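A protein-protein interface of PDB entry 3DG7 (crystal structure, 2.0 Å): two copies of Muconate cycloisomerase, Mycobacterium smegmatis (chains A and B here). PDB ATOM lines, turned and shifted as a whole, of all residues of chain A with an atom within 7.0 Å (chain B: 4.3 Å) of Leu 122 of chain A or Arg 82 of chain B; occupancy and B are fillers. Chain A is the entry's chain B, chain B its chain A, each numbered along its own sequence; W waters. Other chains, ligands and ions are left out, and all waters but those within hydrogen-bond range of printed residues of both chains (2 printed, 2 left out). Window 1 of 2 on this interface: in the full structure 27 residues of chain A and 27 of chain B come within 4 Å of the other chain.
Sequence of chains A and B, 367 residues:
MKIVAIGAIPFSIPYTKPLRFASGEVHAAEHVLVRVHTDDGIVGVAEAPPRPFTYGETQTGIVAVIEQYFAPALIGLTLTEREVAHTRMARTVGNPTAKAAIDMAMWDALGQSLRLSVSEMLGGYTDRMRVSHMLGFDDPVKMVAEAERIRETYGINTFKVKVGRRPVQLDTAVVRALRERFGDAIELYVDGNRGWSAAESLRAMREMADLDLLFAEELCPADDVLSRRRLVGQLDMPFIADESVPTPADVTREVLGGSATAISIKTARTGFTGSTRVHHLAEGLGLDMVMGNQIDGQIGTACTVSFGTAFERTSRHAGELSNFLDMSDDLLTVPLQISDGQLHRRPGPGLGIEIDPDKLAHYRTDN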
ATOM      1  N   ARG A  82     -15.799  18.543   4.022  1.00  0.00           N
ATOM      2  CA  ARG A  82     -14.366  18.299   4.150  1.00  0.00           C
ATOM      3  C   ARG A  82     -13.924  16.951   3.585  1.00  0.00           C
ATOM      4  O   ARG A  82     -12.860  16.852   2.973  1.00  0.00           O
ATOM      5  CB  ARG A  82     -13.937  18.412   5.623  1.00  0.00           C
ATOM      6  CG  ARG A  82     -13.991  19.833   6.178  1.00  0.00           C
ATOM      7  CD  ARG A  82     -13.574  19.910   7.654  1.00  0.00           C
ATOM      8  NE  ARG A  82     -14.457  19.125   8.513  1.00  0.00           N
ATOM      9  CZ  ARG A  82     -14.188  17.898   8.944  1.00  0.00           C
ATOM     10  NH1 ARG A  82     -13.046  17.304   8.612  1.00  0.00           N
ATOM     11  NH2 ARG A  82     -15.077  17.253   9.687  1.00  0.00           N
ATOM     12  N   TRP A 107     -10.946  25.131   7.422  1.00  0.00           N
ATOM     13  CA  TRP A 107     -11.341  25.061   8.829  1.00  0.00           C
ATOM     14  C   TRP A 107     -11.420  26.464   9.437  1.00  0.00           C
ATOM     15  O   TRP A 107     -12.259  26.735  10.300  1.00  0.00           O
ATOM     16  CB  TRP A 107     -10.336  24.230   9.639  1.00  0.00           C
ATOM     17  CG  TRP A 107     -10.573  22.752   9.610  1.00  0.00           C
ATOM     18  CD1 TRP A 107     -10.054  21.848   8.726  1.00  0.00           C
ATOM     19  CD2 TRP A 107     -11.376  22.000  10.524  1.00  0.00           C
ATOM     20  NE1 TRP A 107     -10.479  20.579   9.039  1.00  0.00           N
ATOM     21  CE2 TRP A 107     -11.293  20.644  10.138  1.00  0.00           C
ATOM     22  CE3 TRP A 107     -12.160  22.343  11.635  1.00  0.00           C
ATOM     23  CZ2 TRP A 107     -11.962  19.628  10.823  1.00  0.00           C
ATOM     24  CZ3 TRP A 107     -12.828  21.331  12.319  1.00  0.00           C
ATOM     25  CH2 TRP A 107     -12.723  19.988  11.908  1.00  0.00           C
ATOM     26  N   SER A 117     -13.635  28.493  17.572  1.00  0.00           N
ATOM     27  CA  SER A 117     -12.213  28.330  17.304  1.00  0.00           C
ATOM     28  C   SER A 117     -12.007  26.943  16.706  1.00  0.00           C
ATOM     29  O   SER A 117     -12.797  26.028  16.942  1.00  0.00           O
ATOM     30  CB  SER A 117     -11.407  28.437  18.598  1.00  0.00           C
ATOM     31  OG  SER A 117     -11.718  27.359  19.466  1.00  0.00           O
ATOM     32  N   VAL A 118     -10.950  26.796  15.922  1.00  0.00           N
ATOM     33  CA  VAL A 118     -10.629  25.509  15.325  1.00  0.00           C
ATOM     34  C   VAL A 118     -10.363  24.513  16.453  1.00  0.00           C
ATOM     35  O   VAL A 118     -10.810  23.369  16.400  1.00  0.00           O
ATOM     36  CB  VAL A 118      -9.365  25.614  14.431  1.00  0.00           C
ATOM     37  CG1 VAL A 118      -8.889  24.232  14.020  1.00  0.00           C
ATOM     38  CG2 VAL A 118      -9.681  26.443  13.201  1.00  0.00           C
ATOM     39  N   SER A 119      -9.640  24.965  17.476  1.00  0.00           N
ATOM     40  CA  SER A 119      -9.305  24.109  18.611  1.00  0.00           C
ATOM     41  C   SER A 119     -10.531  23.462  19.250  1.00  0.00           C
ATOM     42  O   SER A 119     -10.569  22.247  19.438  1.00  0.00           O
ATOM     43  CB  SER A 119      -8.539  24.906  19.671  1.00  0.00           C
ATOM     44  OG  SER A 119      -8.228  24.092  20.796  1.00  0.00           O
ATOM     45  N   GLU A 120     -11.546  24.260  19.573  1.00  0.00           N
ATOM     46  CA  GLU A 120     -12.723  23.681  20.203  1.00  0.00           C
ATOM     47  C   GLU A 120     -13.507  22.785  19.250  1.00  0.00           C
ATOM     48  O   GLU A 120     -14.023  21.750  19.666  1.00  0.00           O
ATOM     49  CB  GLU A 120     -13.619  24.778  20.812  1.00  0.00           C
ATOM     50  CG  GLU A 120     -14.318  25.701  19.834  1.00  0.00           C
ATOM     51  CD  GLU A 120     -15.017  26.855  20.549  1.00  0.00           C
ATOM     52  OE1 GLU A 120     -15.875  26.588  21.418  1.00  0.00           O
ATOM     53  OE2 GLU A 120     -14.704  28.025  20.244  1.00  0.00           O
ATOM     54  N   MET A 121     -13.580  23.147  17.972  1.00  0.00           N
ATOM     55  CA  MET A 121     -14.303  22.300  17.019  1.00  0.00           C
ATOM     56  C   MET A 121     -13.628  20.928  16.898  1.00  0.00           C
ATOM     57  O   MET A 121     -14.296  19.923  16.681  1.00  0.00           O
ATOM     58  CB  MET A 121     -14.359  22.943  15.628  1.00  0.00           C
ATOM     59  CG  MET A 121     -15.188  24.215  15.548  1.00  0.00           C
ATOM     60  SD  MET A 121     -15.433  24.753  13.840  1.00  0.00           S
ATOM     61  CE  MET A 121     -13.816  25.391  13.456  1.00  0.00           C
ATOM     62  N   LEU A 122     -12.304  20.899  17.037  1.00  0.00           N
ATOM     63  CA  LEU A 122     -11.543  19.651  16.932  1.00  0.00           C
ATOM     64  C   LEU A 122     -11.636  18.762  18.173  1.00  0.00           C
ATOM     65  O   LEU A 122     -11.420  17.553  18.085  1.00  0.00           O
ATOM     66  CB  LEU A 122     -10.067  19.953  16.634  1.00  0.00           C
ATOM     67  CG  LEU A 122      -9.743  20.466  15.226  1.00  0.00           C
ATOM     68  CD1 LEU A 122      -8.285  20.891  15.150  1.00  0.00           C
ATOM     69  CD2 LEU A 122     -10.049  19.378  14.207  1.00  0.00           C
ATOM     70  N   GLY A 123     -11.953  19.350  19.325  1.00  0.00           N
ATOM     71  CA  GLY A 123     -12.056  18.558  20.542  1.00  0.00           C
ATOM     72  C   GLY A 123     -12.001  19.375  21.820  1.00  0.00           C
ATOM     73  O   GLY A 123     -12.537  18.967  22.854  1.00  0.00           O
ATOM     74  N   GLY A 124     -11.335  20.523  21.743  1.00  0.00           N
ATOM     75  CA  GLY A 124     -11.212  21.426  22.873  1.00  0.00           C
ATOM     76  C   GLY A 124     -10.731  20.840  24.187  1.00  0.00           C
ATOM     77  O   GLY A 124     -11.234  21.221  25.248  1.00  0.00           O
ATOM     78  N   TYR A 125      -9.750  19.939  24.142  1.00  0.00           N
ATOM     79  CA  TYR A 125      -9.255  19.340  25.375  1.00  0.00           C
ATOM     80  C   TYR A 125      -8.692  20.364  26.350  1.00  0.00           C
ATOM     81  O   TYR A 125      -9.012  20.333  27.539  1.00  0.00           O
ATOM     82  CB  TYR A 125      -8.171  18.292  25.111  1.00  0.00           C
ATOM     83  CG  TYR A 125      -7.790  17.563  26.383  1.00  0.00           C
ATOM     84  CD1 TYR A 125      -8.660  16.644  26.962  1.00  0.00           C
ATOM     85  CD2 TYR A 125      -6.589  17.837  27.039  1.00  0.00           C
ATOM     86  CE1 TYR A 125      -8.351  16.018  28.164  1.00  0.00           C
ATOM     87  CE2 TYR A 125      -6.268  17.214  28.243  1.00  0.00           C
ATOM     88  CZ  TYR A 125      -7.154  16.307  28.797  1.00  0.00           C
ATOM     89  OH  TYR A 125      -6.852  15.689  29.983  1.00  0.00           O
ATOM     90  N   GLY A 271      -2.370  19.144   7.880  1.00  0.00           N
ATOM     91  CA  GLY A 271      -3.460  20.052   8.220  1.00  0.00           C
ATOM     92  C   GLY A 271      -4.225  19.662   9.471  1.00  0.00           C
ATOM     93  O   GLY A 271      -3.625  19.297  10.475  1.00  0.00           O
ATOM     94  N   PHE A 272      -5.549  19.751   9.419  1.00  0.00           N
ATOM     95  CA  PHE A 272      -6.363  19.380  10.569  1.00  0.00           C
ATOM     96  C   PHE A 272      -7.090  18.077  10.294  1.00  0.00           C
ATOM     97  O   PHE A 272      -7.106  17.180  11.135  1.00  0.00           O
ATOM     98  CB  PHE A 272      -7.364  20.495  10.917  1.00  0.00           C
ATOM     99  CG  PHE A 272      -6.709  21.809  11.265  1.00  0.00           C
ATOM    100  CD1 PHE A 272      -5.561  21.841  12.055  1.00  0.00           C
ATOM    101  CD2 PHE A 272      -7.246  23.012  10.814  1.00  0.00           C
ATOM    102  CE1 PHE A 272      -4.957  23.047  12.392  1.00  0.00           C
ATOM    103  CE2 PHE A 272      -6.652  24.229  11.146  1.00  0.00           C
ATOM    104  CZ  PHE A 272      -5.503  24.250  11.937  1.00  0.00           C
ATOM    105  N   THR A 273      -7.687  17.964   9.113  1.00  0.00           N
ATOM    106  CA  THR A 273      -8.402  16.750   8.749  1.00  0.00           C
ATOM    107  C   THR A 273      -7.420  15.578   8.698  1.00  0.00           C
ATOM    108  O   THR A 273      -7.683  14.506   9.246  1.00  0.00           O
ATOM    109  CB  THR A 273      -9.095  16.901   7.372  1.00  0.00           C
ATOM    110  OG1 THR A 273     -10.047  17.972   7.435  1.00  0.00           O
ATOM    111  CG2 THR A 273      -9.816  15.620   6.990  1.00  0.00           C
ATOM    112  N   THR A 276      -5.879  14.696  12.162  1.00  0.00           N
ATOM    113  CA  THR A 276      -6.786  13.946  13.020  1.00  0.00           C
ATOM    114  C   THR A 276      -6.632  12.464  12.675  1.00  0.00           C
ATOM    115  O   THR A 276      -6.666  11.605  13.559  1.00  0.00           O
ATOM    116  CB  THR A 276      -8.261  14.370  12.822  1.00  0.00           C
ATOM    117  OG1 THR A 276      -8.414  15.762  13.146  1.00  0.00           O
ATOM    118  CG2 THR A 276      -9.174  13.549  13.733  1.00  0.00           C
ATOM    119  N   HIS A 280      -5.467   9.738  15.503  1.00  0.00           N
ATOM    120  CA  HIS A 280      -6.280   8.573  15.822  1.00  0.00           C
ATOM    121  C   HIS A 280      -5.562   7.262  15.516  1.00  0.00           C
ATOM    122  O   HIS A 280      -5.738   6.268  16.225  1.00  0.00           O
ATOM    123  CB  HIS A 280      -7.620   8.642  15.080  1.00  0.00           C
ATOM    124  CG  HIS A 280      -8.538   9.705  15.607  1.00  0.00           C
ATOM    125  ND1 HIS A 280      -9.840   9.851  15.177  1.00  0.00           N
ATOM    126  CD2 HIS A 280      -8.339  10.670  16.536  1.00  0.00           C
ATOM    127  CE1 HIS A 280     -10.404  10.857  15.819  1.00  0.00           C
ATOM    128  NE2 HIS A 280      -9.516  11.372  16.651  1.00  0.00           N
ATOM    129  N   CYS A 303      -1.756  27.357  13.661  1.00  0.00           N
ATOM    130  CA  CYS A 303      -2.405  26.113  13.257  1.00  0.00           C
ATOM    131  C   CYS A 303      -1.937  24.967  14.148  1.00  0.00           C
ATOM    132  O   CYS A 303      -2.735  24.130  14.580  1.00  0.00           O
ATOM    133  CB  CYS A 303      -2.074  25.786  11.798  1.00  0.00           C
ATOM    134  SG  CYS A 303      -2.875  26.858  10.587  1.00  0.00           S
ATOM    135  N   SER A 306      -3.583  25.186  17.466  1.00  0.00           N
ATOM    136  CA  SER A 306      -5.018  24.933  17.334  1.00  0.00           C
ATOM    137  C   SER A 306      -5.311  23.434  17.421  1.00  0.00           C
ATOM    138  O   SER A 306      -6.248  23.006  18.108  1.00  0.00           O
ATOM    139  CB  SER A 306      -5.554  25.465  15.994  1.00  0.00           C
ATOM    140  OG  SER A 306      -5.672  26.880  16.002  1.00  0.00           O
ATOM    141  N   PHE A 307      -4.516  22.639  16.711  1.00  0.00           N
ATOM    142  CA  PHE A 307      -4.695  21.190  16.702  1.00  0.00           C
ATOM    143  C   PHE A 307      -4.158  20.541  17.982  1.00  0.00           C
ATOM    144  O   PHE A 307      -4.818  19.692  18.584  1.00  0.00           O
ATOM    145  CB  PHE A 307      -3.980  20.573  15.493  1.00  0.00           C
ATOM    146  CG  PHE A 307      -4.193  19.093  15.359  1.00  0.00           C
ATOM    147  CD1 PHE A 307      -5.300  18.595  14.682  1.00  0.00           C
ATOM    148  CD2 PHE A 307      -3.318  18.195  15.967  1.00  0.00           C
ATOM    149  CE1 PHE A 307      -5.540  17.223  14.613  1.00  0.00           C
ATOM    150  CE2 PHE A 307      -3.546  16.822  15.907  1.00  0.00           C
ATOM    151  CZ  PHE A 307      -4.662  16.334  15.227  1.00  0.00           C
ATOM    152  N   GLY A 308      -2.957  20.943  18.385  1.00  0.00           N
ATOM    153  CA  GLY A 308      -2.331  20.381  19.573  1.00  0.00           C
ATOM    154  C   GLY A 308      -3.114  20.501  20.872  1.00  0.00           C
ATOM    155  O   GLY A 308      -3.055  19.608  21.717  1.00  0.00           O
ATOM    156  N   ALA A 310      -6.357  20.588  21.067  1.00  0.00           N
ATOM    157  CA  ALA A 310      -7.628  19.888  20.948  1.00  0.00           C
ATOM    158  C   ALA A 310      -7.671  18.480  21.537  1.00  0.00           C
ATOM    159  O   ALA A 310      -8.747  17.990  21.879  1.00  0.00           O
ATOM    160  CB  ALA A 310      -8.055  19.844  19.485  1.00  0.00           C
ATOM    161  N   PHE A 311      -6.507  17.843  21.657  1.00  0.00           N
ATOM    162  CA  PHE A 311      -6.420  16.477  22.172  1.00  0.00           C
ATOM    163  C   PHE A 311      -5.453  16.333  23.345  1.00  0.00           C
ATOM    164  O   PHE A 311      -4.487  17.084  23.468  1.00  0.00           O
ATOM    165  CB  PHE A 311      -5.965  15.534  21.057  1.00  0.00           C
ATOM    166  CG  PHE A 311      -6.878  15.515  19.870  1.00  0.00           C
ATOM    167  CD1 PHE A 311      -8.035  14.745  19.876  1.00  0.00           C
ATOM    168  CD2 PHE A 311      -6.587  16.281  18.744  1.00  0.00           C
ATOM    169  CE1 PHE A 311      -8.894  14.737  18.776  1.00  0.00           C
ATOM    170  CE2 PHE A 311      -7.433  16.280  17.642  1.00  0.00           C
ATOM    171  CZ  PHE A 311      -8.590  15.506  17.658  1.00  0.00           C
ATOM    172  N   LEU B  79     -20.496  22.080  24.652  1.00  0.00           N
ATOM    173  CA  LEU B  79     -20.616  21.101  23.586  1.00  0.00           C
ATOM    174  C   LEU B  79     -19.372  21.070  22.698  1.00  0.00           C
ATOM    175  O   LEU B  79     -19.279  20.249  21.792  1.00  0.00           O
ATOM    176  CB  LEU B  79     -21.863  21.381  22.744  1.00  0.00           C
ATOM    177  CG  LEU B  79     -23.198  21.296  23.494  1.00  0.00           C
ATOM    178  CD1 LEU B  79     -24.340  21.575  22.530  1.00  0.00           C
ATOM    179  CD2 LEU B  79     -23.357  19.915  24.119  1.00  0.00           C
ATOM    180  N   THR B  80     -18.420  21.965  22.953  1.00  0.00           N
ATOM    181  CA  THR B  80     -17.192  21.983  22.167  1.00  0.00           C
ATOM    182  C   THR B  80     -15.987  21.558  23.011  1.00  0.00           C
ATOM    183  O   THR B  80     -14.863  22.045  22.829  1.00  0.00           O
ATOM    184  CB  THR B  80     -16.930  23.370  21.537  1.00  0.00           C
ATOM    185  OG1 THR B  80     -16.962  24.381  22.551  1.00  0.00           O
ATOM    186  CG2 THR B  80     -17.986  23.672  20.476  1.00  0.00           C
ATOM    187  N   GLU B  81     -16.247  20.648  23.944  1.00  0.00           N
ATOM    188  CA  GLU B  81     -15.215  20.087  24.803  1.00  0.00           C
ATOM    189  C   GLU B  81     -15.387  18.572  24.760  1.00  0.00           C
ATOM    190  O   GLU B  81     -15.264  17.894  25.776  1.00  0.00           O
ATOM    191  CB  GLU B  81     -15.364  20.595  26.243  1.00  0.00           C
ATOM    192  CG  GLU B  81     -14.983  22.058  26.413  1.00  0.00           C
ATOM    193  CD  GLU B  81     -15.016  22.507  27.860  1.00  0.00           C
ATOM    194  OE1 GLU B  81     -16.108  22.520  28.459  1.00  0.00           O
ATOM    195  OE2 GLU B  81     -13.944  22.847  28.398  1.00  0.00           O
ATOM    196  N   ARG B  82     -15.677  18.052  23.570  1.00  0.00           N
ATOM    197  CA  ARG B  82     -15.877  16.619  23.389  1.00  0.00           C
ATOM    198  C   ARG B  82     -14.706  15.769  23.889  1.00  0.00           C
ATOM    199  O   ARG B  82     -14.911  14.699  24.464  1.00  0.00           O
ATOM    200  CB  ARG B  82     -16.152  16.300  21.911  1.00  0.00           C
ATOM    201  CG  ARG B  82     -17.506  16.802  21.413  1.00  0.00           C
ATOM    202  CD  ARG B  82     -17.744  16.483  19.933  1.00  0.00           C
ATOM    203  NE  ARG B  82     -16.756  17.124  19.071  1.00  0.00           N
ATOM    204  CZ  ARG B  82     -15.681  16.517  18.579  1.00  0.00           C
ATOM    205  NH1 ARG B  82     -15.449  15.236  18.850  1.00  0.00           N
ATOM    206  NH2 ARG B  82     -14.824  17.201  17.832  1.00  0.00           N
ATOM    207  N   GLU B  83     -13.482  16.238  23.682  1.00  0.00           N
ATOM    208  CA  GLU B  83     -12.326  15.465  24.125  1.00  0.00           C
ATOM    209  C   GLU B  83     -12.195  15.409  25.643  1.00  0.00           C
ATOM    210  O   GLU B  83     -11.619  14.463  26.182  1.00  0.00           O
ATOM    211  CB  GLU B  83     -11.046  15.998  23.478  1.00  0.00           C
ATOM    212  CG  GLU B  83     -10.923  15.590  22.010  1.00  0.00           C
ATOM    213  CD  GLU B  83     -10.939  14.073  21.818  1.00  0.00           C
ATOM    214  OE1 GLU B  83     -10.212  13.370  22.551  1.00  0.00           O
ATOM    215  OE2 GLU B  83     -11.670  13.583  20.930  1.00  0.00           O
ATOM    216  N   VAL B  84     -12.731  16.414  26.332  1.00  0.00           N
ATOM    217  CA  VAL B  84     -12.706  16.423  27.793  1.00  0.00           C
ATOM    218  C   VAL B  84     -13.729  15.383  28.241  1.00  0.00           C
ATOM    219  O   VAL B  84     -13.466  14.574  29.127  1.00  0.00           O
ATOM    220  CB  VAL B  84     -13.117  17.794  28.377  1.00  0.00           C
ATOM    221  CG1 VAL B  84     -13.115  17.727  29.903  1.00  0.00           C
ATOM    222  CG2 VAL B  84     -12.161  18.872  27.902  1.00  0.00           C
ATOM    223  N   ALA B  85     -14.899  15.408  27.612  1.00  0.00           N
ATOM    224  CA  ALA B  85     -15.948  14.453  27.936  1.00  0.00           C
ATOM    225  C   ALA B  85     -15.453  13.037  27.629  1.00  0.00           C
ATOM    226  O   ALA B  85     -15.651  12.112  28.419  1.00  0.00           O
ATOM    227  CB  ALA B  85     -17.193  14.754  27.122  1.00  0.00           C
ATOM    228  N   HIS B  86     -14.803  12.880  26.479  1.00  0.00           N
ATOM    229  CA  HIS B  86     -14.282  11.582  26.053  1.00  0.00           C
ATOM    230  C   HIS B  86     -13.299  11.036  27.083  1.00  0.00           C
ATOM    231  O   HIS B  86     -13.385   9.873  27.480  1.00  0.00           O
ATOM    232  CB  HIS B  86     -13.597  11.721  24.680  1.00  0.00           C
ATOM    233  CG  HIS B  86     -13.133  10.423  24.093  1.00  0.00           C
ATOM    234  ND1 HIS B  86     -11.833   9.974  24.204  1.00  0.00           N
ATOM    235  CD2 HIS B  86     -13.800   9.468  23.402  1.00  0.00           C
ATOM    236  CE1 HIS B  86     -11.719   8.801  23.607  1.00  0.00           C
ATOM    237  NE2 HIS B  86     -12.898   8.471  23.111  1.00  0.00           N
ATOM    238  N   TRP B 107     -23.506  15.520  20.284  1.00  0.00           N
ATOM    239  CA  TRP B 107     -23.358  15.930  18.888  1.00  0.00           C
ATOM    240  C   TRP B 107     -24.691  16.447  18.329  1.00  0.00           C
ATOM    241  O   TRP B 107     -24.721  17.356  17.496  1.00  0.00           O
ATOM    242  CB  TRP B 107     -22.890  14.756  18.021  1.00  0.00           C
ATOM    243  CG  TRP B 107     -21.410  14.542  18.002  1.00  0.00           C
ATOM    244  CD1 TRP B 107     -20.679  13.745  18.836  1.00  0.00           C
ATOM    245  CD2 TRP B 107     -20.478  15.118  17.079  1.00  0.00           C
ATOM    246  NE1 TRP B 107     -19.348  13.781  18.485  1.00  0.00           N
ATOM    247  CE2 TRP B 107     -19.197  14.618  17.412  1.00  0.00           C
ATOM    248  CE3 TRP B 107     -20.602  16.007  16.003  1.00  0.00           C
ATOM    249  CZ2 TRP B 107     -18.046  14.977  16.705  1.00  0.00           C
ATOM    250  CZ3 TRP B 107     -19.455  16.367  15.300  1.00  0.00           C
ATOM    251  CH2 TRP B 107     -18.193  15.851  15.655  1.00  0.00           C
ATOM    252  N   THR B 273     -17.694  10.342  18.233  1.00  0.00           N
ATOM    253  CA  THR B 273     -16.312  10.652  18.569  1.00  0.00           C
ATOM    254  C   THR B 273     -15.488   9.363  18.542  1.00  0.00           C
ATOM    255  O   THR B 273     -14.412   9.315  17.944  1.00  0.00           O
ATOM    256  CB  THR B 273     -16.215  11.302  19.964  1.00  0.00           C
ATOM    257  OG1 THR B 273     -16.960  12.528  19.968  1.00  0.00           O
ATOM    258  CG2 THR B 273     -14.764  11.597  20.320  1.00  0.00           C
HETATM  259  O   HOH W   1     -12.811  11.422  17.296  1.00  0.00           O
HETATM  260  O   HOH W   2     -12.633  14.563  18.576  1.00  0.00           O
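OE1 of Glu 120 of chain A lies within hydrogen-bond range of OG1 of Thr 80 of chain B, 2.7 Å away.
N of Arg 82 of chain B lies within hydrogen-bond range of O of Gly 123 of chain A, 3.3 Å away.
The backbone carbonyl oxygen (O) of Gly 123 of chain A is in hydrogen-bond range of the backbone NH (N) of Glu 83 of chain B (3.0 Å).
O of Leu 122 of chain A sits at hydrogen-bond distance from NH2 of Arg 82 of chain B.
The guanidinium group (NH2) of Arg 82 of chain B lies within hydrogen-bond range of the backbone carbonyl oxygen (O) of Met 121 of chain A, 3.0 Å away.
The backbone NH (N) of Gly 124 of chain A is in hydrogen-bond range of the backbone carbonyl oxygen (O) of Ser 119 of chain A, 3.0 Å away.
The side-chain carboxylate (OE2) of Glu 120 of chain A sits at hydrogen-bond distance from the backbone NH (N) of Ser 117 of chain A, 2.9 Å away.
NH1 of Arg 82 of chain B lies within hydrogen-bond range of OG1 of Thr 273 of chain B (3.3 Å).
N of Tyr 125 of chain A sits at hydrogen-bond distance from O of Ala 310 of chain A (3.2 Å).
Among the printed residues, pairs that only touch across the chains: Ala 310 of chain A with Glu 83 of chain B, Gly 123 of chain A with Glu 81 of chain B, Tyr 125 of chain A with Val 84 of chain B, Phe 311 of chain A with Glu 83 of chain B, Gly 124 of chain A with Val 84 of chain B, Gly 124 of chain A with Thr 80 of chain B, Tyr 125 of chain A with Glu 83 of chain B and Gly 123 of chain A with Thr 80 of chain B.
Leu 122 of chain A touches one residue of chain B.
Arg 82 of chain B touches just these residues of chain A: Met 121 (3.0 Å), Leu 122 (3.4 Å) and Gly 123 (3.3 Å).
Printed residues of chain A within 4 Å of Glu 83 of chain B: Gly 123, Tyr 125, Ala 310 and Phe 311.
Printed residues of chain B within 4 Å of Phe 311 of chain A: Glu 83 (3.6 Å).
Printed residues of chain B within 4 Å of Ala 310 of chain A: Glu 83 (3.2 Å).
The nearest printed residue of chain B that does not touch Phe 311 of chain A is Arg 82 of chain B (6.5 Å).
Of the 10 printed residues of chain B, 5 touch a printed residue of chain A.
Hydrophobic or aromatic side chains of chain B that line the printed part of chain A: Val 84.
Of the 22 printed residues of chain A, 8 touch a printed residue of chain B.
Printed residues of chain A that touch a printed residue of chain B: Glu 120, Met 121, Leu 122, Gly 123, Gly 124, Tyr 125, Ala 310 and Phe 311.
Among the printed residues, 13 pairs touch across the chains.
3 positions are printed for both chains.
Water W1 bridges O of Thr 273 of chain B (2.7 Å) and NE2 of His 280 of chain A (3.4 Å).
Water W2 lies within hydrogen-bond range of the side-chain carboxylate (OE2) of Glu 83 of chain B (2.7 Å), the guanidinium group (NH1) of Arg 82 of chain B (2.9 Å) and the backbone carbonyl oxygen (O) of Leu 122 of chain A (3.3 Å).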
